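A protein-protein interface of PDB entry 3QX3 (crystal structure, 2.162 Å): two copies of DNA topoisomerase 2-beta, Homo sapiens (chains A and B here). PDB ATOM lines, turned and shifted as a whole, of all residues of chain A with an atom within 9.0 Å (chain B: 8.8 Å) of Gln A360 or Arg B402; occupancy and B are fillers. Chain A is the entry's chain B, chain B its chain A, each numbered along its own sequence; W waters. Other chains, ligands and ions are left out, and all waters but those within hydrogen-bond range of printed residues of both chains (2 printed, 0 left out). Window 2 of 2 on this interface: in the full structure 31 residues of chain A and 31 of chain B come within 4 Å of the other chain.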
ATOM      1  N   VAL A 342     -20.077  10.216 -14.646  1.00  0.00           N
ATOM      2  CA  VAL A 342     -20.977  10.075 -15.793  1.00  0.00           C
ATOM      3  C   VAL A 342     -20.274  10.434 -17.112  1.00  0.00           C
ATOM      4  O   VAL A 342     -20.376   9.706 -18.104  1.00  0.00           O
ATOM      5  CB  VAL A 342     -22.289  10.897 -15.612  1.00  0.00           C
ATOM      6  CG1 VAL A 342     -23.089  10.944 -16.920  1.00  0.00           C
ATOM      7  CG2 VAL A 342     -23.146  10.307 -14.470  1.00  0.00           C
ATOM      8  N   ALA A 343     -19.555  11.551 -17.124  1.00  0.00           N
ATOM      9  CA  ALA A 343     -18.812  11.964 -18.322  1.00  0.00           C
ATOM     10  C   ALA A 343     -17.797  10.908 -18.722  1.00  0.00           C
ATOM     11  O   ALA A 343     -17.594  10.643 -19.910  1.00  0.00           O
ATOM     12  CB  ALA A 343     -18.126  13.323 -18.093  1.00  0.00           C
ATOM     13  N   ALA A 346     -19.667   7.878 -20.255  1.00  0.00           N
ATOM     14  CA  ALA A 346     -20.101   8.252 -21.600  1.00  0.00           C
ATOM     15  C   ALA A 346     -18.953   8.103 -22.622  1.00  0.00           C
ATOM     16  O   ALA A 346     -19.128   7.519 -23.699  1.00  0.00           O
ATOM     17  CB  ALA A 346     -20.650   9.681 -21.591  1.00  0.00           C
ATOM     18  N   GLY A 347     -17.771   8.607 -22.281  1.00  0.00           N
ATOM     19  CA  GLY A 347     -16.609   8.429 -23.146  1.00  0.00           C
ATOM     20  C   GLY A 347     -16.310   6.961 -23.366  1.00  0.00           C
ATOM     21  O   GLY A 347     -16.003   6.518 -24.474  1.00  0.00           O
ATOM     22  N   ALA A 350     -19.014   5.387 -25.786  1.00  0.00           N
ATOM     23  CA  ALA A 350     -18.765   5.764 -27.173  1.00  0.00           C
ATOM     24  C   ALA A 350     -17.680   4.897 -27.812  1.00  0.00           C
ATOM     25  O   ALA A 350     -17.763   4.524 -28.981  1.00  0.00           O
ATOM     26  CB  ALA A 350     -18.374   7.241 -27.252  1.00  0.00           C
ATOM     27  N   TYR A 355     -20.805   4.199 -30.493  1.00  0.00           N
ATOM     28  CA  TYR A 355     -21.833   5.227 -30.494  1.00  0.00           C
ATOM     29  C   TYR A 355     -21.351   6.403 -31.342  1.00  0.00           C
ATOM     30  O   TYR A 355     -20.300   6.970 -31.072  1.00  0.00           O
ATOM     31  CB  TYR A 355     -22.098   5.681 -29.068  1.00  0.00           C
ATOM     32  CG  TYR A 355     -23.147   6.759 -28.910  1.00  0.00           C
ATOM     33  CD1 TYR A 355     -22.778   8.081 -28.692  1.00  0.00           C
ATOM     34  CD2 TYR A 355     -24.510   6.448 -28.923  1.00  0.00           C
ATOM     35  CE1 TYR A 355     -23.716   9.057 -28.510  1.00  0.00           C
ATOM     36  CE2 TYR A 355     -25.465   7.429 -28.740  1.00  0.00           C
ATOM     37  CZ  TYR A 355     -25.058   8.729 -28.544  1.00  0.00           C
ATOM     38  OH  TYR A 355     -25.971   9.715 -28.357  1.00  0.00           O
ATOM     39  N   HIS A 357     -22.564   9.569 -32.047  1.00  0.00           N
ATOM     40  CA  HIS A 357     -23.220  10.848 -31.854  1.00  0.00           C
ATOM     41  C   HIS A 357     -22.486  11.601 -30.781  1.00  0.00           C
ATOM     42  O   HIS A 357     -21.507  11.110 -30.230  1.00  0.00           O
ATOM     43  CB  HIS A 357     -24.686  10.646 -31.455  1.00  0.00           C
ATOM     44  CG  HIS A 357     -25.478   9.861 -32.452  1.00  0.00           C
ATOM     45  ND1 HIS A 357     -25.926  10.402 -33.640  1.00  0.00           N
ATOM     46  CD2 HIS A 357     -25.895   8.572 -32.445  1.00  0.00           C
ATOM     47  CE1 HIS A 357     -26.598   9.484 -34.313  1.00  0.00           C
ATOM     48  NE2 HIS A 357     -26.592   8.363 -33.612  1.00  0.00           N
ATOM     49  N   GLY A 358     -22.960  12.801 -30.480  1.00  0.00           N
ATOM     50  CA  GLY A 358     -22.324  13.613 -29.474  1.00  0.00           C
ATOM     51  C   GLY A 358     -22.433  12.994 -28.100  1.00  0.00           C
ATOM     52  O   GLY A 358     -23.503  12.535 -27.700  1.00  0.00           O
ATOM     53  N   GLU A 359     -21.328  12.993 -27.361  1.00  0.00           N
ATOM     54  CA  GLU A 359     -21.321  12.411 -26.024  1.00  0.00           C
ATOM     55  C   GLU A 359     -22.201  13.138 -24.991  1.00  0.00           C
ATOM     56  O   GLU A 359     -22.548  12.566 -23.965  1.00  0.00           O
ATOM     57  CB  GLU A 359     -19.883  12.241 -25.526  1.00  0.00           C
ATOM     58  CG  GLU A 359     -19.115  11.212 -26.358  1.00  0.00           C
ATOM     59  CD  GLU A 359     -17.785  10.802 -25.740  1.00  0.00           C
ATOM     60  OE1 GLU A 359     -16.958  11.683 -25.435  1.00  0.00           O
ATOM     61  OE2 GLU A 359     -17.566   9.584 -25.563  1.00  0.00           O
ATOM     62  N   GLN A 360     -22.552  14.393 -25.253  1.00  0.00           N
ATOM     63  CA  GLN A 360     -23.450  15.112 -24.357  1.00  0.00           C
ATOM     64  C   GLN A 360     -24.859  14.497 -24.331  1.00  0.00           C
ATOM     65  O   GLN A 360     -25.521  14.517 -23.295  1.00  0.00           O
ATOM     66  CB  GLN A 360     -23.524  16.590 -24.735  1.00  0.00           C
ATOM     67  CG  GLN A 360     -22.196  17.318 -24.637  1.00  0.00           C
ATOM     68  CD  GLN A 360     -21.659  17.384 -23.222  1.00  0.00           C
ATOM     69  OE1 GLN A 360     -22.424  17.418 -22.252  1.00  0.00           O
ATOM     70  NE2 GLN A 360     -20.333  17.412 -23.095  1.00  0.00           N
ATOM     71  N   ALA A 361     -25.317  13.961 -25.465  1.00  0.00           N
ATOM     72  CA  ALA A 361     -26.621  13.287 -25.528  1.00  0.00           C
ATOM     73  C   ALA A 361     -26.550  11.990 -24.710  1.00  0.00           C
ATOM     74  O   ALA A 361     -27.458  11.652 -23.964  1.00  0.00           O
ATOM     75  CB  ALA A 361     -27.018  12.986 -26.983  1.00  0.00           C
ATOM     76  N   LEU A 362     -25.431  11.295 -24.843  1.00  0.00           N
ATOM     77  CA  LEU A 362     -25.161  10.089 -24.095  1.00  0.00           C
ATOM     78  C   LEU A 362     -25.174  10.326 -22.591  1.00  0.00           C
ATOM     79  O   LEU A 362     -25.729   9.527 -21.829  1.00  0.00           O
ATOM     80  CB  LEU A 362     -23.807   9.519 -24.522  1.00  0.00           C
ATOM     81  CG  LEU A 362     -23.640   8.015 -24.369  1.00  0.00           C
ATOM     82  CD1 LEU A 362     -24.862   7.301 -24.943  1.00  0.00           C
ATOM     83  CD2 LEU A 362     -22.358   7.580 -25.066  1.00  0.00           C
ATOM     84  N   MET A 363     -24.568  11.424 -22.158  1.00  0.00           N
ATOM     85  CA  MET A 363     -24.556  11.774 -20.742  1.00  0.00           C
ATOM     86  C   MET A 363     -25.954  12.069 -20.204  1.00  0.00           C
ATOM     87  O   MET A 363     -26.281  11.709 -19.076  1.00  0.00           O
ATOM     88  CB  MET A 363     -23.645  12.979 -20.506  1.00  0.00           C
ATOM     89  CG  MET A 363     -22.176  12.668 -20.839  1.00  0.00           C
ATOM     90  SD  MET A 363     -21.084  14.103 -20.713  1.00  0.00           S
ATOM     91  CE  MET A 363     -19.663  13.543 -21.670  1.00  0.00           C
ATOM     92  N   MET A 364     -26.769  12.762 -20.994  1.00  0.00           N
ATOM     93  CA  MET A 364     -28.169  12.943 -20.624  1.00  0.00           C
ATOM     94  C   MET A 364     -28.921  11.600 -20.556  1.00  0.00           C
ATOM     95  O   MET A 364     -29.761  11.383 -19.684  1.00  0.00           O
ATOM     96  CB  MET A 364     -28.860  13.906 -21.594  1.00  0.00           C
ATOM     97  CG  MET A 364     -28.263  15.306 -21.577  1.00  0.00           C
ATOM     98  SD  MET A 364     -29.180  16.456 -22.614  1.00  0.00           S
ATOM     99  CE  MET A 364     -30.616  16.783 -21.562  1.00  0.00           C
ATOM    100  N   THR A 365     -28.621  10.697 -21.477  1.00  0.00           N
ATOM    101  CA  THR A 365     -29.277   9.395 -21.462  1.00  0.00           C
ATOM    102  C   THR A 365     -28.905   8.655 -20.188  1.00  0.00           C
ATOM    103  O   THR A 365     -29.757   8.013 -19.578  1.00  0.00           O
ATOM    104  CB  THR A 365     -28.901   8.571 -22.679  1.00  0.00           C
ATOM    105  OG1 THR A 365     -29.434   9.201 -23.847  1.00  0.00           O
ATOM    106  CG2 THR A 365     -29.438   7.137 -22.557  1.00  0.00           C
ATOM    107  N   ILE A 366     -27.639   8.773 -19.779  1.00  0.00           N
ATOM    108  CA  ILE A 366     -27.155   8.126 -18.572  1.00  0.00           C
ATOM    109  C   ILE A 366     -27.822   8.700 -17.329  1.00  0.00           C
ATOM    110  O   ILE A 366     -28.277   7.954 -16.457  1.00  0.00           O
ATOM    111  CB  ILE A 366     -25.614   8.224 -18.425  1.00  0.00           C
ATOM    112  CG1 ILE A 366     -24.917   7.366 -19.488  1.00  0.00           C
ATOM    113  CG2 ILE A 366     -25.203   7.793 -17.029  1.00  0.00           C
ATOM    114  CD1 ILE A 366     -23.444   7.730 -19.721  1.00  0.00           C
ATOM    115  N   VAL A 367     -27.914  10.019 -17.257  1.00  0.00           N
ATOM    116  CA  VAL A 367     -28.645  10.667 -16.173  1.00  0.00           C
ATOM    117  C   VAL A 367     -30.097  10.157 -16.105  1.00  0.00           C
ATOM    118  O   VAL A 367     -30.620   9.869 -15.022  1.00  0.00           O
ATOM    119  CB  VAL A 367     -28.620  12.215 -16.305  1.00  0.00           C
ATOM    120  CG1 VAL A 367     -29.665  12.850 -15.400  1.00  0.00           C
ATOM    121  CG2 VAL A 367     -27.232  12.748 -15.978  1.00  0.00           C
ATOM    122  N   SER A 400     -23.933  18.882 -13.280  1.00  0.00           N
ATOM    123  CA  SER A 400     -23.195  18.591 -14.489  1.00  0.00           C
ATOM    124  C   SER A 400     -22.693  17.160 -14.425  1.00  0.00           C
ATOM    125  O   SER A 400     -22.354  16.679 -13.346  1.00  0.00           O
ATOM    126  CB  SER A 400     -22.014  19.559 -14.600  1.00  0.00           C
ATOM    127  OG  SER A 400     -21.081  19.139 -15.573  1.00  0.00           O
ATOM    128  N   PRO A 401     -22.655  16.471 -15.576  1.00  0.00           N
ATOM    129  CA  PRO A 401     -22.202  15.074 -15.662  1.00  0.00           C
ATOM    130  C   PRO A 401     -20.722  14.884 -15.352  1.00  0.00           C
ATOM    131  O   PRO A 401     -20.245  13.750 -15.251  1.00  0.00           O
ATOM    132  CB  PRO A 401     -22.507  14.683 -17.115  1.00  0.00           C
ATOM    133  CG  PRO A 401     -22.768  15.957 -17.827  1.00  0.00           C
ATOM    134  CD  PRO A 401     -23.292  16.920 -16.825  1.00  0.00           C
ATOM    135  N   ARG A 402     -20.002  15.987 -15.201  1.00  0.00           N
ATOM    136  CA  ARG A 402     -18.604  15.934 -14.786  1.00  0.00           C
ATOM    137  C   ARG A 402     -18.512  15.827 -13.266  1.00  0.00           C
ATOM    138  O   ARG A 402     -17.472  15.488 -12.722  1.00  0.00           O
ATOM    139  CB  ARG A 402     -17.847  17.175 -15.277  1.00  0.00           C
ATOM    140  CG  ARG A 402     -17.780  17.321 -16.796  1.00  0.00           C
ATOM    141  CD  ARG A 402     -17.007  18.578 -17.212  1.00  0.00           C
ATOM    142  NE  ARG A 402     -17.875  19.608 -17.781  1.00  0.00           N
ATOM    143  CZ  ARG A 402     -18.212  20.735 -17.160  1.00  0.00           C
ATOM    144  NH1 ARG A 402     -17.746  20.988 -15.944  1.00  0.00           N
ATOM    145  NH2 ARG A 402     -19.008  21.612 -17.760  1.00  0.00           N
ATOM    146  N   VAL B 340      -6.249   8.006 -27.020  1.00  0.00           N
ATOM    147  CA  VAL B 340      -7.289   8.177 -26.016  1.00  0.00           C
ATOM    148  C   VAL B 340      -7.786   9.626 -26.039  1.00  0.00           C
ATOM    149  O   VAL B 340      -6.979  10.562 -26.151  1.00  0.00           O
ATOM    150  CB  VAL B 340      -6.725   7.838 -24.620  1.00  0.00           C
ATOM    151  CG1 VAL B 340      -7.679   8.254 -23.524  1.00  0.00           C
ATOM    152  CG2 VAL B 340      -6.393   6.343 -24.527  1.00  0.00           C
ATOM    153  N   LYS B 341      -9.099   9.822 -25.936  1.00  0.00           N
ATOM    154  CA  LYS B 341      -9.645  11.180 -25.895  1.00  0.00           C
ATOM    155  C   LYS B 341      -9.037  11.963 -24.742  1.00  0.00           C
ATOM    156  O   LYS B 341      -8.901  11.440 -23.626  1.00  0.00           O
ATOM    157  CB  LYS B 341     -11.171  11.164 -25.737  1.00  0.00           C
ATOM    158  CG  LYS B 341     -11.926  11.800 -26.875  1.00  0.00           C
ATOM    159  CD  LYS B 341     -13.432  11.665 -26.621  1.00  0.00           C
ATOM    160  CE  LYS B 341     -14.244  11.577 -27.912  1.00  0.00           C
ATOM    161  NZ  LYS B 341     -15.511  10.786 -27.708  1.00  0.00           N
ATOM    162  N   VAL B 342      -8.692  13.221 -24.995  1.00  0.00           N
ATOM    163  CA  VAL B 342      -8.076  14.037 -23.951  1.00  0.00           C
ATOM    164  C   VAL B 342      -8.991  14.153 -22.727  1.00  0.00           C
ATOM    165  O   VAL B 342      -8.551  13.991 -21.571  1.00  0.00           O
ATOM    166  CB  VAL B 342      -7.678  15.438 -24.489  1.00  0.00           C
ATOM    167  CG1 VAL B 342      -7.329  16.367 -23.328  1.00  0.00           C
ATOM    168  CG2 VAL B 342      -6.497  15.314 -25.475  1.00  0.00           C
ATOM    169  N   ALA B 343     -10.277  14.401 -22.970  1.00  0.00           N
ATOM    170  CA  ALA B 343     -11.221  14.528 -21.857  1.00  0.00           C
ATOM    171  C   ALA B 343     -11.231  13.250 -21.027  1.00  0.00           C
ATOM    172  O   ALA B 343     -11.257  13.295 -19.805  1.00  0.00           O
ATOM    173  CB  ALA B 343     -12.642  14.877 -22.366  1.00  0.00           C
ATOM    174  N   GLN B 344     -11.172  12.108 -21.709  1.00  0.00           N
ATOM    175  CA  GLN B 344     -11.207  10.810 -21.055  1.00  0.00           C
ATOM    176  C   GLN B 344      -9.913  10.523 -20.280  1.00  0.00           C
ATOM    177  O   GLN B 344      -9.953  10.002 -19.155  1.00  0.00           O
ATOM    178  CB  GLN B 344     -11.459   9.724 -22.111  1.00  0.00           C
ATOM    179  CG  GLN B 344     -11.765   8.344 -21.563  1.00  0.00           C
ATOM    180  CD  GLN B 344     -13.212   8.212 -21.102  1.00  0.00           C
ATOM    181  OE1 GLN B 344     -14.008   9.158 -21.210  1.00  0.00           O
ATOM    182  NE2 GLN B 344     -13.561   7.038 -20.583  1.00  0.00           N
ATOM    183  N   GLN B 360     -11.026  20.394 -16.012  1.00  0.00           N
ATOM    184  CA  GLN B 360     -10.771  21.286 -17.136  1.00  0.00           C
ATOM    185  C   GLN B 360      -9.335  21.839 -17.109  1.00  0.00           C
ATOM    186  O   GLN B 360      -8.729  22.020 -18.166  1.00  0.00           O
ATOM    187  CB  GLN B 360     -11.804  22.412 -17.224  1.00  0.00           C
ATOM    188  CG  GLN B 360     -13.226  21.934 -17.528  1.00  0.00           C
ATOM    189  CD  GLN B 360     -13.351  21.231 -18.874  1.00  0.00           C
ATOM    190  OE1 GLN B 360     -12.815  21.697 -19.883  1.00  0.00           O
ATOM    191  NE2 GLN B 360     -14.064  20.101 -18.892  1.00  0.00           N
ATOM    192  N   MET B 363      -7.191  19.019 -18.493  1.00  0.00           N
ATOM    193  CA  MET B 363      -7.271  18.907 -19.937  1.00  0.00           C
ATOM    194  C   MET B 363      -6.390  19.954 -20.618  1.00  0.00           C
ATOM    195  O   MET B 363      -5.773  19.673 -21.640  1.00  0.00           O
ATOM    196  CB  MET B 363      -8.717  19.002 -20.428  1.00  0.00           C
ATOM    197  CG  MET B 363      -9.602  17.805 -20.019  1.00  0.00           C
ATOM    198  SD  MET B 363     -11.348  18.174 -20.311  1.00  0.00           S
ATOM    199  CE  MET B 363     -12.116  17.277 -18.941  1.00  0.00           C
ATOM    200  N   VAL B 367      -3.165  19.213 -23.108  1.00  0.00           N
ATOM    201  CA  VAL B 367      -3.002  19.852 -24.410  1.00  0.00           C
ATOM    202  C   VAL B 367      -1.615  20.508 -24.535  1.00  0.00           C
ATOM    203  O   VAL B 367      -0.951  20.423 -25.582  1.00  0.00           O
ATOM    204  CB  VAL B 367      -4.118  20.901 -24.684  1.00  0.00           C
ATOM    205  CG1 VAL B 367      -3.700  21.888 -25.746  1.00  0.00           C
ATOM    206  CG2 VAL B 367      -5.416  20.194 -25.109  1.00  0.00           C
ATOM    207  N   ALA B 399      -8.740  22.639 -30.606  1.00  0.00           N
ATOM    208  CA  ALA B 399     -10.141  22.242 -30.534  1.00  0.00           C
ATOM    209  C   ALA B 399     -10.429  21.792 -29.112  1.00  0.00           C
ATOM    210  O   ALA B 399      -9.522  21.705 -28.276  1.00  0.00           O
ATOM    211  CB  ALA B 399     -10.439  21.128 -31.511  1.00  0.00           C
ATOM    212  N   SER B 400     -11.694  21.509 -28.841  1.00  0.00           N
ATOM    213  CA  SER B 400     -12.118  21.080 -27.521  1.00  0.00           C
ATOM    214  C   SER B 400     -11.498  19.731 -27.151  1.00  0.00           C
ATOM    215  O   SER B 400     -11.349  18.852 -28.005  1.00  0.00           O
ATOM    216  CB  SER B 400     -13.654  20.987 -27.471  1.00  0.00           C
ATOM    217  OG  SER B 400     -14.058  20.207 -26.359  1.00  0.00           O
ATOM    218  N   PRO B 401     -11.157  19.557 -25.870  1.00  0.00           N
ATOM    219  CA  PRO B 401     -10.573  18.303 -25.376  1.00  0.00           C
ATOM    220  C   PRO B 401     -11.492  17.094 -25.543  1.00  0.00           C
ATOM    221  O   PRO B 401     -11.037  15.957 -25.424  1.00  0.00           O
ATOM    222  CB  PRO B 401     -10.325  18.589 -23.880  1.00  0.00           C
ATOM    223  CG  PRO B 401     -11.163  19.754 -23.559  1.00  0.00           C
ATOM    224  CD  PRO B 401     -11.220  20.582 -24.816  1.00  0.00           C
ATOM    225  N   ARG B 402     -12.777  17.316 -25.797  1.00  0.00           N
ATOM    226  CA  ARG B 402     -13.669  16.193 -26.038  1.00  0.00           C
ATOM    227  C   ARG B 402     -13.561  15.683 -27.473  1.00  0.00           C
ATOM    228  O   ARG B 402     -14.093  14.633 -27.797  1.00  0.00           O
ATOM    229  CB  ARG B 402     -15.116  16.560 -25.694  1.00  0.00           C
ATOM    230  CG  ARG B 402     -15.329  16.850 -24.211  1.00  0.00           C
ATOM    231  CD  ARG B 402     -16.018  18.187 -24.006  1.00  0.00           C
ATOM    232  NE  ARG B 402     -17.338  18.209 -24.628  1.00  0.00           N
ATOM    233  CZ  ARG B 402     -17.990  19.318 -24.946  1.00  0.00           C
ATOM    234  NH1 ARG B 402     -17.451  20.504 -24.703  1.00  0.00           N
ATOM    235  NH2 ARG B 402     -19.183  19.245 -25.508  1.00  0.00           N
ATOM    236  N   TYR B 403     -12.854  16.421 -28.322  1.00  0.00           N
ATOM    237  CA  TYR B 403     -12.731  16.047 -29.731  1.00  0.00           C
ATOM    238  C   TYR B 403     -11.311  15.708 -30.177  1.00  0.00           C
ATOM    239  O   TYR B 403     -11.086  15.451 -31.361  1.00  0.00           O
ATOM    240  CB  TYR B 403     -13.219  17.167 -30.636  1.00  0.00           C
ATOM    241  CG  TYR B 403     -14.621  17.640 -30.374  1.00  0.00           C
ATOM    242  CD1 TYR B 403     -15.630  16.753 -29.987  1.00  0.00           C
ATOM    243  CD2 TYR B 403     -14.936  18.979 -30.501  1.00  0.00           C
ATOM    244  CE1 TYR B 403     -16.923  17.210 -29.749  1.00  0.00           C
ATOM    245  CE2 TYR B 403     -16.205  19.442 -30.259  1.00  0.00           C
ATOM    246  CZ  TYR B 403     -17.194  18.563 -29.888  1.00  0.00           C
ATOM    247  OH  TYR B 403     -18.452  19.069 -29.663  1.00  0.00           O
ATOM    248  N   ILE B 404     -10.353  15.740 -29.257  1.00  0.00           N
ATOM    249  CA  ILE B 404      -8.962  15.461 -29.631  1.00  0.00           C
ATOM    250  C   ILE B 404      -8.405  14.299 -28.826  1.00  0.00           C
ATOM    251  O   ILE B 404      -8.926  13.958 -27.758  1.00  0.00           O
ATOM    252  CB  ILE B 404      -8.080  16.711 -29.503  1.00  0.00           C
ATOM    253  CG1 ILE B 404      -8.164  17.300 -28.087  1.00  0.00           C
ATOM    254  CG2 ILE B 404      -8.497  17.735 -30.532  1.00  0.00           C
ATOM    255  CD1 ILE B 404      -7.373  18.587 -27.923  1.00  0.00           C
ATOM    256  N   PHE B 405      -7.357  13.681 -29.351  1.00  0.00           N
ATOM    257  CA  PHE B 405      -6.828  12.443 -28.791  1.00  0.00           C
ATOM    258  C   PHE B 405      -5.325  12.560 -28.550  1.00  0.00           C
ATOM    259  O   PHE B 405      -4.641  13.354 -29.187  1.00  0.00           O
ATOM    260  CB  PHE B 405      -7.067  11.274 -29.764  1.00  0.00           C
ATOM    261  CG  PHE B 405      -8.521  11.014 -30.081  1.00  0.00           C
ATOM    262  CD1 PHE B 405      -9.203  11.818 -30.979  1.00  0.00           C
ATOM    263  CD2 PHE B 405      -9.187   9.940 -29.507  1.00  0.00           C
ATOM    264  CE1 PHE B 405     -10.532  11.580 -31.279  1.00  0.00           C
ATOM    265  CE2 PHE B 405     -10.515   9.694 -29.804  1.00  0.00           C
ATOM    266  CZ  PHE B 405     -11.187  10.517 -30.692  1.00  0.00           C
HETATM  267  O   HOH W   1     -14.589  11.115 -23.908  1.00  0.00           O
HETATM  268  O   HOH W   2     -14.786  11.626 -21.123  1.00  0.00           O
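NH2 of Arg B402 lies close to NE2 of Gln A360, 3.2 Å away. The side-chain amino group (NZ) of Lys B341 is in salt-bridge range of the side-chain carboxylate (OE1) of Glu A359 (2.8 Å).
Gln A360 touches Arg B402, and with the chains exchanged Arg A402 touches Gln B360.
Among the printed residues, merely in contact across the chains: Gly A347 with Gln B344 and Arg A402 with Gln B360.
Water W2 lies within hydrogen-bond range of OE1 of Gln B344 (2.6 Å) and O of Ala A343 (3.2 Å). Water W1 lies within hydrogen-bond range of OE1 of Glu A359 (2.9 Å) and OE1 of Gln B344 (3.4 Å).
Printed residues of chain B within 4 Å of Gly A347: Gln B344 (3.3 Å). Printed residues of chain B within 4 Å of Glu A359: Lys B341. Of the printed residues of chain B, Gln A360 touches Arg B402. Pro A401 touches none of the printed residues of chain B. Of the printed residues of chain B, Arg A402 touches Gln B360. Of the printed residues of chain A, Lys B341 touches Glu A359. Of the printed residues of chain A, Gln B344 touches Gly A347 (3.3 Å). Printed residues of chain A within 4 Å of Arg B402: Gln A360. The nearest printed residue of chain A that does not touch Gln B360 is Ser A400 (7.8 Å).
The side-chain sulfur (SD) of Met B363 lies close to the side-chain amide nitrogen (NE2) of Gln B360 (3.6 Å). OE2 of Glu A359 sits close to N of Gly A347, 3.4 Å away. The side-chain hydroxyl of Ser B400 sits close to the backbone NH of Arg B402 (3.2 Å). The side-chain hydroxyl (OG) of Ser A400 lies close to the backbone NH (N) of Arg A402, at 3.4 Å.
Of the 20 printed residues of chain A, 4 touch a printed residue of chain B. Of the 15 printed residues of chain B, 4 touch a printed residue of chain A. Among the printed residues, 4 pairs touch across the chains.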
